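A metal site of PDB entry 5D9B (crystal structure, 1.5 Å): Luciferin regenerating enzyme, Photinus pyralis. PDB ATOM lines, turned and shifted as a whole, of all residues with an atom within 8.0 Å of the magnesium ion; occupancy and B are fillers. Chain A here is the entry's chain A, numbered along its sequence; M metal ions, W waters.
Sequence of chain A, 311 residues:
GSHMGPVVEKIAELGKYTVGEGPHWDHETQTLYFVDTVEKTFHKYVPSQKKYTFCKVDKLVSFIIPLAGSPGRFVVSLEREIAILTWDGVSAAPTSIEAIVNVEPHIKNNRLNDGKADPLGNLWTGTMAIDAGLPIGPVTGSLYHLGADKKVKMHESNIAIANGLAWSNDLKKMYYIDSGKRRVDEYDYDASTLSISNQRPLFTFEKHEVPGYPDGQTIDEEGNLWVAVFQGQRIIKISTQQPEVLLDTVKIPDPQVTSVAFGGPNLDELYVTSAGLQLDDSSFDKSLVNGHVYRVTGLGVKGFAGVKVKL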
ATOM      1  N   VAL A  19       5.416  34.208  -1.406  1.00  0.00           N
ATOM      2  CA  VAL A  19       6.357  33.121  -1.634  1.00  0.00           C
ATOM      3  C   VAL A  19       6.632  33.104  -3.151  1.00  0.00           C
ATOM      4  O   VAL A  19       6.022  32.348  -3.916  1.00  0.00           O
ATOM      5  CB  VAL A  19       5.844  31.755  -1.121  1.00  0.00           C
ATOM      6  CG1 VAL A  19       6.942  30.674  -1.321  1.00  0.00           C
ATOM      7  CG2 VAL A  19       5.466  31.805   0.411  1.00  0.00           C
ATOM      8  N   GLY A  20       7.572  33.930  -3.585  1.00  0.00           N
ATOM      9  CA  GLY A  20       8.007  33.860  -4.986  1.00  0.00           C
ATOM     10  C   GLY A  20       8.690  32.517  -5.219  1.00  0.00           C
ATOM     11  O   GLY A  20       9.447  32.073  -4.344  1.00  0.00           O
ATOM     12  N   GLU A  21       8.421  31.850  -6.341  1.00  0.00           N
ATOM     13  CA  GLU A  21       8.905  30.479  -6.534  1.00  0.00           C
ATOM     14  C   GLU A  21       8.916  30.073  -7.983  1.00  0.00           C
ATOM     15  O   GLU A  21       8.378  30.783  -8.812  1.00  0.00           O
ATOM     16  CB  GLU A  21       8.042  29.462  -5.789  1.00  0.00           C
ATOM     17  CG  GLU A  21       8.654  29.038  -4.436  1.00  0.00           C
ATOM     18  CD  GLU A  21       9.772  28.007  -4.569  1.00  0.00           C
ATOM     19  OE1 GLU A  21      10.111  27.414  -3.519  1.00  0.00           O
ATOM     20  OE2 GLU A  21      10.257  27.771  -5.684  1.00  0.00           O
ATOM     21  N   GLY A  22       9.508  28.909  -8.258  1.00  0.00           N
ATOM     22  CA  GLY A  22       9.376  28.261  -9.568  1.00  0.00           C
ATOM     23  C   GLY A  22       9.840  29.070 -10.778  1.00  0.00           C
ATOM     24  O   GLY A  22       9.182  29.070 -11.809  1.00  0.00           O
ATOM     25  N   PRO A  23      11.009  29.738 -10.700  1.00  0.00           N
ATOM     26  CA  PRO A  23      11.490  30.476 -11.873  1.00  0.00           C
ATOM     27  C   PRO A  23      11.814  29.582 -13.058  1.00  0.00           C
ATOM     28  O   PRO A  23      12.432  28.511 -12.908  1.00  0.00           O
ATOM     29  CB  PRO A  23      12.751  31.158 -11.362  1.00  0.00           C
ATOM     30  CG  PRO A  23      13.239  30.271 -10.217  1.00  0.00           C
ATOM     31  CD  PRO A  23      11.938  29.887  -9.549  1.00  0.00           C
ATOM     32  N   THR A  37       3.281  31.141  -4.729  1.00  0.00           N
ATOM     33  CA  THR A  37       2.442  30.015  -4.342  1.00  0.00           C
ATOM     34  C   THR A  37       1.203  30.492  -3.594  1.00  0.00           C
ATOM     35  O   THR A  37       0.064  30.171  -3.989  1.00  0.00           O
ATOM     36  CB  THR A  37       3.221  28.996  -3.498  1.00  0.00           C
ATOM     37  OG1 THR A  37       3.755  29.634  -2.330  1.00  0.00           O
ATOM     38  CG2 THR A  37       4.361  28.413  -4.295  1.00  0.00           C
ATOM     39  N   SER A  62       2.339  26.128  -7.925  1.00  0.00           N
ATOM     40  CA  SER A  62       3.745  25.967  -7.554  1.00  0.00           C
ATOM     41  C   SER A  62       4.731  25.912  -8.728  1.00  0.00           C
ATOM     42  O   SER A  62       5.928  25.992  -8.512  1.00  0.00           O
ATOM     43  CB  SER A  62       3.903  24.706  -6.688  1.00  0.00           C
ATOM     44  OG  SER A  62       3.574  23.516  -7.392  1.00  0.00           O
ATOM     45  N   ARG A 111      -0.692  19.182  -1.378  1.00  0.00           N
ATOM     46  CA  ARG A 111      -0.558  20.000  -2.563  1.00  0.00           C
ATOM     47  C   ARG A 111       0.716  19.648  -3.313  1.00  0.00           C
ATOM     48  O   ARG A 111       1.659  19.113  -2.744  1.00  0.00           O
ATOM     49  CB  ARG A 111      -0.537  21.488  -2.183  1.00  0.00           C
ATOM     50  CG  ARG A 111       0.751  21.961  -1.537  1.00  0.00           C
ATOM     51  CD  ARG A 111       0.936  23.463  -1.729  1.00  0.00           C
ATOM     52  NE  ARG A 111       1.921  24.085  -0.847  1.00  0.00           N
ATOM     53  CZ  ARG A 111       3.124  24.496  -1.244  1.00  0.00           C
ATOM     54  NH1 ARG A 111       3.943  25.081  -0.387  1.00  0.00           N
ATOM     55  NH2 ARG A 111       3.494  24.334  -2.510  1.00  0.00           N
ATOM     56  N   ASN A 113       4.244  20.716  -4.947  1.00  0.00           N
ATOM     57  CA  ASN A 113       5.201  21.783  -4.734  1.00  0.00           C
ATOM     58  C   ASN A 113       6.151  21.852  -5.920  1.00  0.00           C
ATOM     59  O   ASN A 113       5.677  21.983  -7.054  1.00  0.00           O
ATOM     60  CB  ASN A 113       5.943  21.617  -3.406  1.00  0.00           C
ATOM     61  CG  ASN A 113       6.625  22.906  -2.968  1.00  0.00           C
ATOM     62  OD1 ASN A 113       6.187  24.005  -3.301  1.00  0.00           O
ATOM     63  ND2 ASN A 113       7.699  22.781  -2.229  1.00  0.00           N
ATOM     64  N   ASP A 114       7.469  21.779  -5.722  1.00  0.00           N
ATOM     65  CA  ASP A 114       8.381  22.103  -6.838  1.00  0.00           C
ATOM     66  C   ASP A 114       8.216  21.091  -7.993  1.00  0.00           C
ATOM     67  O   ASP A 114       7.907  19.916  -7.788  1.00  0.00           O
ATOM     68  CB  ASP A 114       9.861  22.143  -6.403  1.00  0.00           C
ATOM     69  CG  ASP A 114      10.675  23.160  -7.206  1.00  0.00           C
ATOM     70  OD1 ASP A 114      10.164  23.715  -8.199  1.00  0.00           O
ATOM     71  OD2 ASP A 114      11.833  23.429  -6.834  1.00  0.00           O
ATOM     72  N   GLY A 115       8.422  21.571  -9.208  1.00  0.00           N
ATOM     73  CA  GLY A 115       8.325  20.709 -10.382  1.00  0.00           C
ATOM     74  C   GLY A 115       9.214  21.259 -11.479  1.00  0.00           C
ATOM     75  O   GLY A 115       9.446  22.465 -11.566  1.00  0.00           O
ATOM     76  N   MET A 128       3.305  17.496  -0.876  1.00  0.00           N
ATOM     77  CA  MET A 128       3.605  17.789   0.535  1.00  0.00           C
ATOM     78  C   MET A 128       2.302  18.168   1.216  1.00  0.00           C
ATOM     79  O   MET A 128       1.358  18.637   0.562  1.00  0.00           O
ATOM     80  CB  MET A 128       4.596  18.939   0.623  1.00  0.00           C
ATOM     81  CG  MET A 128       4.099  20.255  -0.023  1.00  0.00           C
ATOM     82  SD  MET A 128       5.298  21.604   0.183  1.00  0.00           S
ATOM     83  CE  MET A 128       4.898  22.149   1.840  1.00  0.00           C
ATOM     84  N   ILE A 161       8.904  18.018   2.487  1.00  0.00           N
ATOM     85  CA  ILE A 161       8.714  19.210   1.664  1.00  0.00           C
ATOM     86  C   ILE A 161       9.421  18.980   0.322  1.00  0.00           C
ATOM     87  O   ILE A 161      10.634  19.102   0.179  1.00  0.00           O
ATOM     88  CB  ILE A 161       9.228  20.489   2.355  1.00  0.00           C
ATOM     89  CG1 ILE A 161       8.509  20.655   3.725  1.00  0.00           C
ATOM     90  CG2 ILE A 161       9.029  21.715   1.449  1.00  0.00           C
ATOM     91  CD1 ILE A 161       8.779  21.977   4.431  1.00  0.00           C
ATOM     92  N   ALA A 162       8.636  18.604  -0.671  1.00  0.00           N
ATOM     93  CA  ALA A 162       9.141  18.245  -1.990  1.00  0.00           C
ATOM     94  C   ALA A 162       9.704  19.464  -2.691  1.00  0.00           C
ATOM     95  O   ALA A 162       8.964  20.421  -3.035  1.00  0.00           O
ATOM     96  CB  ALA A 162       8.010  17.606  -2.815  1.00  0.00           C
ATOM     97  N   ASN A 163      11.010  19.489  -2.895  1.00  0.00           N
ATOM     98  CA  ASN A 163      11.575  20.724  -3.434  1.00  0.00           C
ATOM     99  C   ASN A 163      12.509  20.498  -4.619  1.00  0.00           C
ATOM    100  O   ASN A 163      12.128  19.795  -5.549  1.00  0.00           O
ATOM    101  CB  ASN A 163      12.218  21.535  -2.289  1.00  0.00           C
ATOM    102  CG  ASN A 163      11.444  22.789  -2.025  1.00  0.00           C
ATOM    103  OD1 ASN A 163      10.932  23.392  -2.979  1.00  0.00           O
ATOM    104  ND2 ASN A 163      11.303  23.186  -0.745  1.00  0.00           N
ATOM    105  N   GLY A 164      13.669  21.142  -4.633  1.00  0.00           N
ATOM    106  CA  GLY A 164      14.380  21.322  -5.897  1.00  0.00           C
ATOM    107  C   GLY A 164      14.854  20.051  -6.608  1.00  0.00           C
ATOM    108  O   GLY A 164      15.171  19.065  -5.966  1.00  0.00           O
ATOM    109  N   ILE A 177      15.875  17.455  -3.533  1.00  0.00           N
ATOM    110  CA  ILE A 177      15.818  18.065  -2.204  1.00  0.00           C
ATOM    111  C   ILE A 177      14.475  17.875  -1.530  1.00  0.00           C
ATOM    112  O   ILE A 177      13.449  18.304  -2.036  1.00  0.00           O
ATOM    113  CB  ILE A 177      16.132  19.589  -2.299  1.00  0.00           C
ATOM    114  CG1 ILE A 177      17.603  19.794  -2.709  1.00  0.00           C
ATOM    115  CG2 ILE A 177      15.778  20.298  -0.984  1.00  0.00           C
ATOM    116  CD1 ILE A 177      17.861  21.229  -3.185  1.00  0.00           C
ATOM    117  N   SER A 179      13.327  19.390   1.721  1.00  0.00           N
ATOM    118  CA  SER A 179      13.836  20.423   2.636  1.00  0.00           C
ATOM    119  C   SER A 179      13.916  19.967   4.093  1.00  0.00           C
ATOM    120  O   SER A 179      14.797  20.430   4.844  1.00  0.00           O
ATOM    121  CB  SER A 179      12.953  21.681   2.550  1.00  0.00           C
ATOM    122  OG  SER A 179      13.006  22.250   1.237  1.00  0.00           O
ATOM    123  N   PRO A 214      17.598  23.778   2.433  1.00  0.00           N
ATOM    124  CA  PRO A 214      17.675  23.847   0.975  1.00  0.00           C
ATOM    125  C   PRO A 214      16.277  23.914   0.370  1.00  0.00           C
ATOM    126  O   PRO A 214      15.354  23.282   0.882  1.00  0.00           O
ATOM    127  CB  PRO A 214      18.392  22.525   0.586  1.00  0.00           C
ATOM    128  CG  PRO A 214      17.958  21.555   1.717  1.00  0.00           C
ATOM    129  CD  PRO A 214      17.870  22.425   2.982  1.00  0.00           C
ATOM    130  N   ASP A 215      16.120  24.634  -0.731  1.00  0.00           N
ATOM    131  CA  ASP A 215      14.770  24.819  -1.302  1.00  0.00           C
ATOM    132  C   ASP A 215      14.890  24.456  -2.784  1.00  0.00           C
ATOM    133  O   ASP A 215      14.987  23.268  -3.112  1.00  0.00           O
ATOM    134  CB  ASP A 215      14.295  26.244  -1.034  1.00  0.00           C
ATOM    135  CG  ASP A 215      12.785  26.431  -1.231  1.00  0.00           C
ATOM    136  OD1 ASP A 215      12.194  25.753  -2.074  1.00  0.00           O
ATOM    137  OD2 ASP A 215      12.221  27.326  -0.545  1.00  0.00           O
ATOM    138  N   GLY A 216      14.930  25.438  -3.686  1.00  0.00           N
ATOM    139  CA  GLY A 216      15.102  25.149  -5.119  1.00  0.00           C
ATOM    140  C   GLY A 216      16.574  24.971  -5.483  1.00  0.00           C
ATOM    141  O   GLY A 216      17.467  25.395  -4.745  1.00  0.00           O
ATOM    142  N   GLN A 217      16.821  24.364  -6.657  1.00  0.00           N
ATOM    143  CA  GLN A 217      18.204  24.220  -7.138  1.00  0.00           C
ATOM    144  C   GLN A 217      18.265  24.180  -8.641  1.00  0.00           C
ATOM    145  O   GLN A 217      17.252  23.890  -9.310  1.00  0.00           O
ATOM    146  CB  GLN A 217      18.849  22.943  -6.547  1.00  0.00           C
ATOM    147  CG  GLN A 217      18.311  21.642  -7.132  1.00  0.00           C
ATOM    148  CD  GLN A 217      19.014  20.457  -6.518  1.00  0.00           C
ATOM    149  OE1 GLN A 217      20.146  20.587  -6.124  1.00  0.00           O
ATOM    150  NE2 GLN A 217      18.315  19.314  -6.398  1.00  0.00           N
ATOM    151  N   ALA A 228      19.296  27.234  -3.429  1.00  0.00           N
ATOM    152  CA  ALA A 228      18.716  28.330  -2.662  1.00  0.00           C
ATOM    153  C   ALA A 228      18.575  27.910  -1.205  1.00  0.00           C
ATOM    154  O   ALA A 228      18.115  26.809  -0.919  1.00  0.00           O
ATOM    155  CB  ALA A 228      17.338  28.705  -3.244  1.00  0.00           C
ATOM    156  N   PHE A 230      16.749  28.715   2.114  1.00  0.00           N
ATOM    157  CA  PHE A 230      15.638  29.368   2.761  1.00  0.00           C
ATOM    158  C   PHE A 230      15.984  29.586   4.238  1.00  0.00           C
ATOM    159  O   PHE A 230      16.352  28.646   4.903  1.00  0.00           O
ATOM    160  CB  PHE A 230      14.379  28.508   2.550  1.00  0.00           C
ATOM    161  CG  PHE A 230      13.121  29.124   3.072  1.00  0.00           C
ATOM    162  CD1 PHE A 230      12.287  29.839   2.215  1.00  0.00           C
ATOM    163  CD2 PHE A 230      12.742  28.965   4.401  1.00  0.00           C
ATOM    164  CE1 PHE A 230      11.092  30.419   2.729  1.00  0.00           C
ATOM    165  CE2 PHE A 230      11.563  29.537   4.876  1.00  0.00           C
ATOM    166  CZ  PHE A 230      10.749  30.250   4.026  1.00  0.00           C
ATOM    167  N   VAL A 257      15.472  32.980   0.718  1.00  0.00           N
ATOM    168  CA  VAL A 257      15.732  32.666  -0.692  1.00  0.00           C
ATOM    169  C   VAL A 257      15.012  31.368  -1.037  1.00  0.00           C
ATOM    170  O   VAL A 257      15.154  30.390  -0.290  1.00  0.00           O
ATOM    171  CB  VAL A 257      17.234  32.483  -0.920  1.00  0.00           C
ATOM    172  CG1 VAL A 257      17.490  32.269  -2.399  1.00  0.00           C
ATOM    173  CG2 VAL A 257      18.012  33.691  -0.380  1.00  0.00           C
ATOM    174  N   THR A 258      14.293  31.302  -2.161  1.00  0.00           N
ATOM    175  CA  THR A 258      13.506  30.101  -2.459  1.00  0.00           C
ATOM    176  C   THR A 258      13.976  29.287  -3.670  1.00  0.00           C
ATOM    177  O   THR A 258      13.908  28.052  -3.644  1.00  0.00           O
ATOM    178  CB  THR A 258      11.999  30.440  -2.706  1.00  0.00           C
ATOM    179  OG1 THR A 258      11.880  31.419  -3.742  1.00  0.00           O
ATOM    180  CG2 THR A 258      11.346  30.986  -1.424  1.00  0.00           C
ATOM    181  N   SER A 259      14.350  29.948  -4.752  1.00  0.00           N
ATOM    182  CA  SER A 259      14.769  29.178  -5.930  1.00  0.00           C
ATOM    183  C   SER A 259      15.622  30.006  -6.889  1.00  0.00           C
ATOM    184  O   SER A 259      15.907  31.195  -6.633  1.00  0.00           O
ATOM    185  CB  SER A 259      13.540  28.624  -6.655  1.00  0.00           C
ATOM    186  OG  SER A 259      13.904  27.547  -7.560  1.00  0.00           O
ATOM    187  N   THR A 273      14.503  33.954  -6.697  1.00  0.00           N
ATOM    188  CA  THR A 273      13.252  34.328  -6.053  1.00  0.00           C
ATOM    189  C   THR A 273      13.394  34.223  -4.521  1.00  0.00           C
ATOM    190  O   THR A 273      14.264  33.514  -3.992  1.00  0.00           O
ATOM    191  CB  THR A 273      12.069  33.407  -6.536  1.00  0.00           C
ATOM    192  OG1 THR A 273      12.439  32.035  -6.352  1.00  0.00           O
ATOM    193  CG2 THR A 273      11.759  33.631  -8.048  1.00  0.00           C
HETATM  194 MG    MG M   1      10.648  25.456  -3.270  1.00  0.00          MG
HETATM  195  O   HOH W   1       8.872  24.924  -4.480  1.00  0.00           O
HETATM  196  O   HOH W   2      11.714  25.554  -4.988  1.00  0.00           O
HETATM  197  O   HOH W   3       9.175  25.392  -1.610  1.00  0.00           O
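The backbone NH of Gly 164 sits at hydrogen-bond distance from the backbone carbonyl oxygen of Asp 215, 2.9 Å away. The backbone carbonyl oxygen (O) of Ala 228 is in hydrogen-bond range of the backbone NH (N) of Asp 215. OD1 of Asn 163 sits close to ND2 of Asn 113, 3.4 Å away. ND2 of Asn 163 is in hydrogen-bond range of OG of Ser 179 (2.8 Å). The backbone carbonyl oxygen of Ile 177 lies within hydrogen-bond range of the backbone NH of Asn 163 (2.8 Å).
Of the 28 residues printed, 3 come within 4 Å of the magnesium ion.
The magnesium ion is bound by the side-chain carboxylate of Asp 215 (2.0 Å), water W2 (2.0 Å), the side-chain carboxylate of Glu 21 (2.0 Å), the side-chain amide oxygen of Asn 163 (2.1 Å), water W1 (2.2 Å) and water W3 (2.2 Å). The magnesium ion has six donor atoms within binding distance.
Water W1 bridges the side-chain amide oxygen of Asn 113 and the side-chain carboxylate of Glu 21. Water W3 bridges the side-chain amide nitrogen (ND2) of Asn 113 (3.1 Å) and the side-chain amide nitrogen (ND2) of Asn 163 (3.2 Å). Water W2 lies within hydrogen-bond range of the side-chain carboxylate of Glu 21 (2.7 Å), the side-chain carboxylate of Asp 114 (2.8 Å) and the backbone NH of Gly 216 (3.5 Å).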
